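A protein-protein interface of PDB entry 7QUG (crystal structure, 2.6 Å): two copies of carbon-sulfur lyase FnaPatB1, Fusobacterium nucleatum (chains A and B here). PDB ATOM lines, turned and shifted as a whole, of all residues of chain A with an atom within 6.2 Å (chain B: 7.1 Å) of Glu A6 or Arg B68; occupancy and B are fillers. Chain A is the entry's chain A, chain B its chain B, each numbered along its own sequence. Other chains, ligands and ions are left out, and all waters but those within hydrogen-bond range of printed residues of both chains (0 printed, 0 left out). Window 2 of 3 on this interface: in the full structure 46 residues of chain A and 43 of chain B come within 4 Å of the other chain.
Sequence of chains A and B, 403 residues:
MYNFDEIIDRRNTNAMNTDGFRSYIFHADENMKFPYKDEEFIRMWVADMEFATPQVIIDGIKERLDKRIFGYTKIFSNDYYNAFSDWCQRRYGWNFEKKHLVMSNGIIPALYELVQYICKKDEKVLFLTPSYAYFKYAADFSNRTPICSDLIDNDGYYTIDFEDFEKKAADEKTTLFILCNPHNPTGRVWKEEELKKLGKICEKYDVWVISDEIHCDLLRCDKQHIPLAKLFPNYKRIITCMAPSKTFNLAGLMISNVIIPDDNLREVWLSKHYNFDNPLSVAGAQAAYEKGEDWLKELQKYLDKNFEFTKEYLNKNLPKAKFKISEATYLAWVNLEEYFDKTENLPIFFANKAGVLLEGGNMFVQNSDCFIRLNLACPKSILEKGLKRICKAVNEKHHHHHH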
ATOM      1  N   ASN A   3      -6.078  -3.818  -8.179  1.00  0.00           N
ATOM      2  CA  ASN A   3      -5.523  -4.906  -7.381  1.00  0.00           C
ATOM      3  C   ASN A   3      -5.647  -4.589  -5.886  1.00  0.00           C
ATOM      4  O   ASN A   3      -4.671  -4.230  -5.221  1.00  0.00           O
ATOM      5  CB  ASN A   3      -4.075  -5.179  -7.801  1.00  0.00           C
ATOM      6  CG  ASN A   3      -3.475  -6.354  -7.062  1.00  0.00           C
ATOM      7  OD1 ASN A   3      -4.207  -7.205  -6.551  1.00  0.00           O
ATOM      8  ND2 ASN A   3      -2.144  -6.428  -7.017  1.00  0.00           N
ATOM      9  N   PHE A   4      -6.857  -4.783  -5.340  1.00  0.00           N
ATOM     10  CA  PHE A   4      -7.076  -4.591  -3.907  1.00  0.00           C
ATOM     11  C   PHE A   4      -6.381  -5.629  -3.039  1.00  0.00           C
ATOM     12  O   PHE A   4      -6.315  -5.441  -1.820  1.00  0.00           O
ATOM     13  CB  PHE A   4      -8.565  -4.600  -3.561  1.00  0.00           C
ATOM     14  CG  PHE A   4      -9.313  -3.409  -4.061  1.00  0.00           C
ATOM     15  CD1 PHE A   4      -9.239  -2.203  -3.383  1.00  0.00           C
ATOM     16  CD2 PHE A   4     -10.129  -3.495  -5.166  1.00  0.00           C
ATOM     17  CE1 PHE A   4      -9.931  -1.093  -3.840  1.00  0.00           C
ATOM     18  CE2 PHE A   4     -10.825  -2.389  -5.615  1.00  0.00           C
ATOM     19  CZ  PHE A   4     -10.725  -1.191  -4.957  1.00  0.00           C
ATOM     20  N   ASP A   5      -5.882  -6.716  -3.616  1.00  0.00           N
ATOM     21  CA  ASP A   5      -5.101  -7.672  -2.845  1.00  0.00           C
ATOM     22  C   ASP A   5      -3.673  -7.214  -2.635  1.00  0.00           C
ATOM     23  O   ASP A   5      -2.947  -7.830  -1.848  1.00  0.00           O
ATOM     24  CB  ASP A   5      -5.097  -9.031  -3.543  1.00  0.00           C
ATOM     25  CG  ASP A   5      -6.456  -9.649  -3.576  1.00  0.00           C
ATOM     26  OD1 ASP A   5      -7.009  -9.914  -2.486  1.00  0.00           O
ATOM     27  OD2 ASP A   5      -6.977  -9.840  -4.693  1.00  0.00           O
ATOM     28  N   GLU A   6      -3.250  -6.177  -3.348  1.00  0.00           N
ATOM     29  CA  GLU A   6      -1.878  -5.707  -3.242  1.00  0.00           C
ATOM     30  C   GLU A   6      -1.597  -5.213  -1.833  1.00  0.00           C
ATOM     31  O   GLU A   6      -2.327  -4.371  -1.300  1.00  0.00           O
ATOM     32  CB  GLU A   6      -1.624  -4.584  -4.241  1.00  0.00           C
ATOM     33  CG  GLU A   6      -0.254  -4.003  -4.102  1.00  0.00           C
ATOM     34  CD  GLU A   6      -0.062  -2.806  -4.975  1.00  0.00           C
ATOM     35  OE1 GLU A   6       1.087  -2.329  -5.061  1.00  0.00           O
ATOM     36  OE2 GLU A   6      -1.066  -2.329  -5.556  1.00  0.00           O
ATOM     37  N   ILE A   7      -0.526  -5.720  -1.243  1.00  0.00           N
ATOM     38  CA  ILE A   7      -0.060  -5.221   0.041  1.00  0.00           C
ATOM     39  C   ILE A   7       0.748  -3.947  -0.172  1.00  0.00           C
ATOM     40  O   ILE A   7       1.578  -3.858  -1.085  1.00  0.00           O
ATOM     41  CB  ILE A   7       0.748  -6.291   0.776  1.00  0.00           C
ATOM     42  CG1 ILE A   7      -0.199  -7.440   1.141  1.00  0.00           C
ATOM     43  CG2 ILE A   7       1.448  -5.668   1.994  1.00  0.00           C
ATOM     44  CD1 ILE A   7       0.467  -8.626   1.786  1.00  0.00           C
ATOM     45  N   ILE A   8       0.480  -2.944   0.655  1.00  0.00           N
ATOM     46  CA  ILE A   8       1.040  -1.610   0.493  1.00  0.00           C
ATOM     47  C   ILE A   8       1.804  -1.268   1.758  1.00  0.00           C
ATOM     48  O   ILE A   8       1.232  -1.282   2.853  1.00  0.00           O
ATOM     49  CB  ILE A   8      -0.054  -0.580   0.190  1.00  0.00           C
ATOM     50  CG1 ILE A   8      -0.529  -0.803  -1.245  1.00  0.00           C
ATOM     51  CG2 ILE A   8       0.477   0.839   0.413  1.00  0.00           C
ATOM     52  CD1 ILE A   8      -1.946  -0.533  -1.459  1.00  0.00           C
ATOM     53  N   GLU A  50      -5.791   0.129   4.201  1.00  0.00           N
ATOM     54  CA  GLU A  50      -4.536  -0.380   3.690  1.00  0.00           C
ATOM     55  C   GLU A  50      -4.485  -0.374   2.164  1.00  0.00           C
ATOM     56  O   GLU A  50      -3.449  -0.728   1.595  1.00  0.00           O
ATOM     57  CB  GLU A  50      -4.297  -1.789   4.229  1.00  0.00           C
ATOM     58  CG  GLU A  50      -4.297  -1.848   5.728  1.00  0.00           C
ATOM     59  CD  GLU A  50      -3.242  -0.946   6.353  1.00  0.00           C
ATOM     60  OE1 GLU A  50      -3.556  -0.204   7.312  1.00  0.00           O
ATOM     61  OE2 GLU A  50      -2.097  -0.957   5.867  1.00  0.00           O
ATOM     62  N   PHE A  51      -5.581  -0.024   1.500  1.00  0.00           N
ATOM     63  CA  PHE A  51      -5.620   0.089   0.052  1.00  0.00           C
ATOM     64  C   PHE A  51      -4.992   1.404  -0.393  1.00  0.00           C
ATOM     65  O   PHE A  51      -5.025   2.402   0.331  1.00  0.00           O
ATOM     66  CB  PHE A  51      -7.063   0.013  -0.445  1.00  0.00           C
ATOM     67  CG  PHE A  51      -7.804  -1.192   0.056  1.00  0.00           C
ATOM     68  CD1 PHE A  51      -7.226  -2.456  -0.007  1.00  0.00           C
ATOM     69  CD2 PHE A  51      -9.082  -1.064   0.612  1.00  0.00           C
ATOM     70  CE1 PHE A  51      -7.910  -3.572   0.458  1.00  0.00           C
ATOM     71  CE2 PHE A  51      -9.766  -2.175   1.080  1.00  0.00           C
ATOM     72  CZ  PHE A  51      -9.181  -3.430   1.001  1.00  0.00           C
ATOM     73  N   ALA A  52      -4.435   1.408  -1.602  1.00  0.00           N
ATOM     74  CA  ALA A  52      -3.870   2.638  -2.142  1.00  0.00           C
ATOM     75  C   ALA A  52      -4.968   3.604  -2.583  1.00  0.00           C
ATOM     76  O   ALA A  52      -6.022   3.200  -3.081  1.00  0.00           O
ATOM     77  CB  ALA A  52      -2.939   2.331  -3.317  1.00  0.00           C
ATOM     78  N   THR A  53      -4.715   4.889  -2.390  1.00  0.00           N
ATOM     79  CA  THR A  53      -5.576   5.900  -2.972  1.00  0.00           C
ATOM     80  C   THR A  53      -5.617   5.707  -4.485  1.00  0.00           C
ATOM     81  O   THR A  53      -4.578   5.419  -5.095  1.00  0.00           O
ATOM     82  CB  THR A  53      -5.039   7.285  -2.619  1.00  0.00           C
ATOM     83  OG1 THR A  53      -5.026   7.408  -1.191  1.00  0.00           O
ATOM     84  CG2 THR A  53      -5.894   8.405  -3.238  1.00  0.00           C
ATOM     85  N   PRO A  54      -6.788   5.824  -5.115  1.00  0.00           N
ATOM     86  CA  PRO A  54      -6.862   5.665  -6.572  1.00  0.00           C
ATOM     87  C   PRO A  54      -5.867   6.570  -7.280  1.00  0.00           C
ATOM     88  O   PRO A  54      -5.687   7.738  -6.919  1.00  0.00           O
ATOM     89  CB  PRO A  54      -8.297   6.072  -6.914  1.00  0.00           C
ATOM     90  CG  PRO A  54      -9.004   6.213  -5.653  1.00  0.00           C
ATOM     91  CD  PRO A  54      -8.069   6.226  -4.518  1.00  0.00           C
ATOM     92  N   GLN A  55      -5.266   6.027  -8.345  1.00  0.00           N
ATOM     93  CA  GLN A  55      -4.253   6.757  -9.095  1.00  0.00           C
ATOM     94  C   GLN A  55      -4.822   8.006  -9.756  1.00  0.00           C
ATOM     95  O   GLN A  55      -4.079   8.971  -9.958  1.00  0.00           O
ATOM     96  CB  GLN A  55      -3.628   5.831 -10.134  1.00  0.00           C
ATOM     97  CG  GLN A  55      -2.412   6.367 -10.891  1.00  0.00           C
ATOM     98  CD  GLN A  55      -1.178   6.526 -10.024  1.00  0.00           C
ATOM     99  OE1 GLN A  55      -0.870   5.675  -9.169  1.00  0.00           O
ATOM    100  NE2 GLN A  55      -0.452   7.621 -10.245  1.00  0.00           N
ATOM    101  N   ILE A  58      -4.247  10.611  -7.139  1.00  0.00           N
ATOM    102  CA  ILE A  58      -2.830  10.944  -7.059  1.00  0.00           C
ATOM    103  C   ILE A  58      -2.401  11.768  -8.270  1.00  0.00           C
ATOM    104  O   ILE A  58      -1.650  12.739  -8.130  1.00  0.00           O
ATOM    105  CB  ILE A  58      -1.966   9.670  -6.920  1.00  0.00           C
ATOM    106  CG1 ILE A  58      -2.318   8.901  -5.638  1.00  0.00           C
ATOM    107  CG2 ILE A  58      -0.468  10.040  -6.951  1.00  0.00           C
ATOM    108  CD1 ILE A  58      -1.363   7.789  -5.282  1.00  0.00           C
ATOM    109  N   ASN A 249      -9.288   7.161   1.356  1.00  0.00           N
ATOM    110  CA  ASN A 249      -8.067   7.116   2.162  1.00  0.00           C
ATOM    111  C   ASN A 249      -7.306   8.446   2.070  1.00  0.00           C
ATOM    112  O   ASN A 249      -6.109   8.503   1.760  1.00  0.00           O
ATOM    113  CB  ASN A 249      -7.178   5.944   1.742  1.00  0.00           C
ATOM    114  CG  ASN A 249      -6.535   5.250   2.915  1.00  0.00           C
ATOM    115  OD1 ASN A 249      -6.627   5.708   4.066  1.00  0.00           O
ATOM    116  ND2 ASN A 249      -5.805   4.174   2.620  1.00  0.00           N
ATOM    117  N   TYR A 302     -15.134  -5.234  -3.212  1.00  0.00           N
ATOM    118  CA  TYR A 302     -14.113  -5.919  -2.433  1.00  0.00           C
ATOM    119  C   TYR A 302     -14.445  -5.910  -0.947  1.00  0.00           C
ATOM    120  O   TYR A 302     -14.197  -6.900  -0.249  1.00  0.00           O
ATOM    121  CB  TYR A 302     -12.754  -5.284  -2.686  1.00  0.00           C
ATOM    122  CG  TYR A 302     -11.585  -6.097  -2.194  1.00  0.00           C
ATOM    123  CD1 TYR A 302     -10.944  -7.020  -3.021  1.00  0.00           C
ATOM    124  CD2 TYR A 302     -11.099  -5.928  -0.913  1.00  0.00           C
ATOM    125  CE1 TYR A 302      -9.856  -7.764  -2.567  1.00  0.00           C
ATOM    126  CE2 TYR A 302     -10.020  -6.651  -0.456  1.00  0.00           C
ATOM    127  CZ  TYR A 302      -9.399  -7.566  -1.287  1.00  0.00           C
ATOM    128  OH  TYR A 302      -8.329  -8.286  -0.811  1.00  0.00           O
ATOM    129  N   PRO A 379      -6.166  -5.956   2.246  1.00  0.00           N
ATOM    130  CA  PRO A 379      -6.266  -7.146   1.381  1.00  0.00           C
ATOM    131  C   PRO A 379      -6.761  -8.364   2.147  1.00  0.00           C
ATOM    132  O   PRO A 379      -6.503  -8.520   3.343  1.00  0.00           O
ATOM    133  CB  PRO A 379      -4.834  -7.333   0.865  1.00  0.00           C
ATOM    134  CG  PRO A 379      -4.279  -5.953   0.868  1.00  0.00           C
ATOM    135  CD  PRO A 379      -4.862  -5.290   2.107  1.00  0.00           C
ATOM    136  N   GLU B  63       7.446  12.263  -4.020  1.00  0.00           N
ATOM    137  CA  GLU B  63       7.960  11.082  -3.348  1.00  0.00           C
ATOM    138  C   GLU B  63       6.983  10.572  -2.285  1.00  0.00           C
ATOM    139  O   GLU B  63       6.772   9.356  -2.159  1.00  0.00           O
ATOM    140  CB  GLU B  63       9.320  11.452  -2.791  1.00  0.00           C
ATOM    141  CG  GLU B  63      10.248  10.357  -2.427  1.00  0.00           C
ATOM    142  CD  GLU B  63      11.588  10.948  -2.068  1.00  0.00           C
ATOM    143  OE1 GLU B  63      12.026  10.781  -0.900  1.00  0.00           O
ATOM    144  OE2 GLU B  63      12.148  11.658  -2.953  1.00  0.00           O
ATOM    145  N   ARG B  64       6.373  11.486  -1.510  1.00  0.00           N
ATOM    146  CA  ARG B  64       5.343  11.072  -0.560  1.00  0.00           C
ATOM    147  C   ARG B  64       4.079  10.620  -1.280  1.00  0.00           C
ATOM    148  O   ARG B  64       3.398   9.686  -0.828  1.00  0.00           O
ATOM    149  CB  ARG B  64       5.010  12.205   0.400  1.00  0.00           C
ATOM    150  CG  ARG B  64       3.877  11.874   1.385  1.00  0.00           C
ATOM    151  CD  ARG B  64       4.139  10.593   2.150  1.00  0.00           C
ATOM    152  NE  ARG B  64       3.121  10.335   3.157  1.00  0.00           N
ATOM    153  CZ  ARG B  64       1.987   9.664   2.938  1.00  0.00           C
ATOM    154  NH1 ARG B  64       1.716   9.176   1.735  1.00  0.00           N
ATOM    155  NH2 ARG B  64       1.119   9.476   3.927  1.00  0.00           N
ATOM    156  N   LEU B  65       3.750  11.277  -2.399  1.00  0.00           N
ATOM    157  CA  LEU B  65       2.625  10.852  -3.227  1.00  0.00           C
ATOM    158  C   LEU B  65       2.756   9.399  -3.644  1.00  0.00           C
ATOM    159  O   LEU B  65       1.758   8.670  -3.730  1.00  0.00           O
ATOM    160  CB  LEU B  65       2.545  11.724  -4.471  1.00  0.00           C
ATOM    161  CG  LEU B  65       1.322  12.585  -4.740  1.00  0.00           C
ATOM    162  CD1 LEU B  65       0.417  12.773  -3.523  1.00  0.00           C
ATOM    163  CD2 LEU B  65       1.811  13.916  -5.249  1.00  0.00           C
ATOM    164  N   ASP B  66       3.988   8.957  -3.901  1.00  0.00           N
ATOM    165  CA  ASP B  66       4.250   7.605  -4.372  1.00  0.00           C
ATOM    166  C   ASP B  66       4.115   6.563  -3.278  1.00  0.00           C
ATOM    167  O   ASP B  66       4.154   5.369  -3.588  1.00  0.00           O
ATOM    168  CB  ASP B  66       5.643   7.521  -4.981  1.00  0.00           C
ATOM    169  CG  ASP B  66       5.786   8.368  -6.259  1.00  0.00           C
ATOM    170  OD1 ASP B  66       4.746   8.714  -6.900  1.00  0.00           O
ATOM    171  OD2 ASP B  66       6.955   8.656  -6.631  1.00  0.00           O
ATOM    172  N   LYS B  67       3.997   6.970  -2.011  1.00  0.00           N
ATOM    173  CA  LYS B  67       3.676   6.003  -0.970  1.00  0.00           C
ATOM    174  C   LYS B  67       2.207   5.608  -1.010  1.00  0.00           C
ATOM    175  O   LYS B  67       1.827   4.639  -0.351  1.00  0.00           O
ATOM    176  CB  LYS B  67       4.038   6.551   0.424  1.00  0.00           C
ATOM    177  CG  LYS B  67       5.493   6.990   0.594  1.00  0.00           C
ATOM    178  CD  LYS B  67       6.442   5.827   0.386  1.00  0.00           C
ATOM    179  CE  LYS B  67       7.845   6.321   0.133  1.00  0.00           C
ATOM    180  NZ  LYS B  67       8.812   5.200  -0.053  1.00  0.00           N
ATOM    181  N   ARG B  68       1.385   6.348  -1.755  1.00  0.00           N
ATOM    182  CA  ARG B  68       0.053   5.979  -2.237  1.00  0.00           C
ATOM    183  C   ARG B  68      -1.060   5.963  -1.191  1.00  0.00           C
ATOM    184  O   ARG B  68      -2.233   5.770  -1.562  1.00  0.00           O
ATOM    185  CB  ARG B  68       0.072   4.617  -2.941  1.00  0.00           C
ATOM    186  CG  ARG B  68       0.818   4.669  -4.257  1.00  0.00           C
ATOM    187  CD  ARG B  68       0.321   3.575  -5.176  1.00  0.00           C
ATOM    188  NE  ARG B  68       0.958   2.318  -4.831  1.00  0.00           N
ATOM    189  CZ  ARG B  68       0.529   1.125  -5.211  1.00  0.00           C
ATOM    190  NH1 ARG B  68       1.207   0.050  -4.824  1.00  0.00           N
ATOM    191  NH2 ARG B  68      -0.567   1.009  -5.952  1.00  0.00           N
ATOM    192  N   ILE B  69      -0.765   6.198   0.084  1.00  0.00           N
ATOM    193  CA  ILE B  69      -1.785   6.225   1.121  1.00  0.00           C
ATOM    194  C   ILE B  69      -1.657   7.539   1.875  1.00  0.00           C
ATOM    195  O   ILE B  69      -0.552   8.062   2.024  1.00  0.00           O
ATOM    196  CB  ILE B  69      -1.677   4.997   2.048  1.00  0.00           C
ATOM    197  CG1 ILE B  69      -2.123   3.743   1.286  1.00  0.00           C
ATOM    198  CG2 ILE B  69      -2.470   5.186   3.340  1.00  0.00           C
ATOM    199  CD1 ILE B  69      -2.296   2.542   2.169  1.00  0.00           C
ATOM    200  N   PHE B  70      -2.795   8.130   2.248  1.00  0.00           N
ATOM    201  CA  PHE B  70      -2.833   9.454   2.869  1.00  0.00           C
ATOM    202  C   PHE B  70      -3.725   9.450   4.110  1.00  0.00           C
ATOM    203  O   PHE B  70      -4.593  10.304   4.297  1.00  0.00           O
ATOM    204  CB  PHE B  70      -3.244  10.489   1.819  1.00  0.00           C
ATOM    205  CG  PHE B  70      -2.442  10.374   0.564  1.00  0.00           C
ATOM    206  CD1 PHE B  70      -1.148  10.895   0.508  1.00  0.00           C
ATOM    207  CD2 PHE B  70      -2.941   9.691  -0.541  1.00  0.00           C
ATOM    208  CE1 PHE B  70      -0.362  10.746  -0.639  1.00  0.00           C
ATOM    209  CE2 PHE B  70      -2.164   9.543  -1.717  1.00  0.00           C
ATOM    210  CZ  PHE B  70      -0.878  10.073  -1.760  1.00  0.00           C
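The side-chain carboxylate (OE2) of Glu A6 is in salt-bridge range of the guanidinium group (NH1) of Arg B68 (3.4 Å).
The backbone carbonyl oxygen of Arg B68 lies within hydrogen-bond range of the backbone NH of Thr A53 (2.8 Å).
The backbone NH (N) of Phe B70 sits at hydrogen-bond distance from the backbone carbonyl oxygen (O) of Asn A249 (3.4 Å).
OD1 of Asn A3 sits at hydrogen-bond distance from N of Glu A6 (3.5 Å).
The side-chain amide nitrogen (ND2) of Asn A249 lies within hydrogen-bond range of the backbone carbonyl oxygen (O) of Phe A51 (3.0 Å).
O of Asn A249 lies within hydrogen-bond range of OG1 of Thr A53, 3.3 Å away.
The backbone carbonyl oxygen (O) of Ile B69 sits at hydrogen-bond distance from the guanidinium group (NH1) of Arg B64 (2.5 Å).
Among the printed residues, pairs that only touch across the chains: Thr A53 with Phe B70, Phe A51 with Ile B69, Glu A50 with Ile B69, Asn A249 with Ile B69, Ala A52 with Arg B68, Ile A58 with Leu B65, Ile A8 with Ile B69, Ile A58 with Arg B68 and Ile A58 with Phe B70.
Printed residues of chain B within 4 Å of Glu A6: Arg B68 (2.4 Å).
Of chain A, only Glu A6 (2.4 Å), Ala A52 (3.6 Å), Thr A53 (2.8 Å) and Ile A58 (3.8 Å) come within 4 Å of Arg B68.
Of the printed residues of chain B, Ala A52 touches Arg B68 (3.6 Å).
Of the printed residues of chain B, Asn A249 touches Ile B69 (3.6 Å) and Phe B70 (3.4 Å).
Tyr A302 touches none of the printed residues of chain B.
Asn A3 touches none of the printed residues of chain B.
Along chain B the printed residues that touch a printed residue of chain A span positions 65 to 70.
Among the printed residues, 12 pairs touch across the chains.
No position is printed for both chains.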
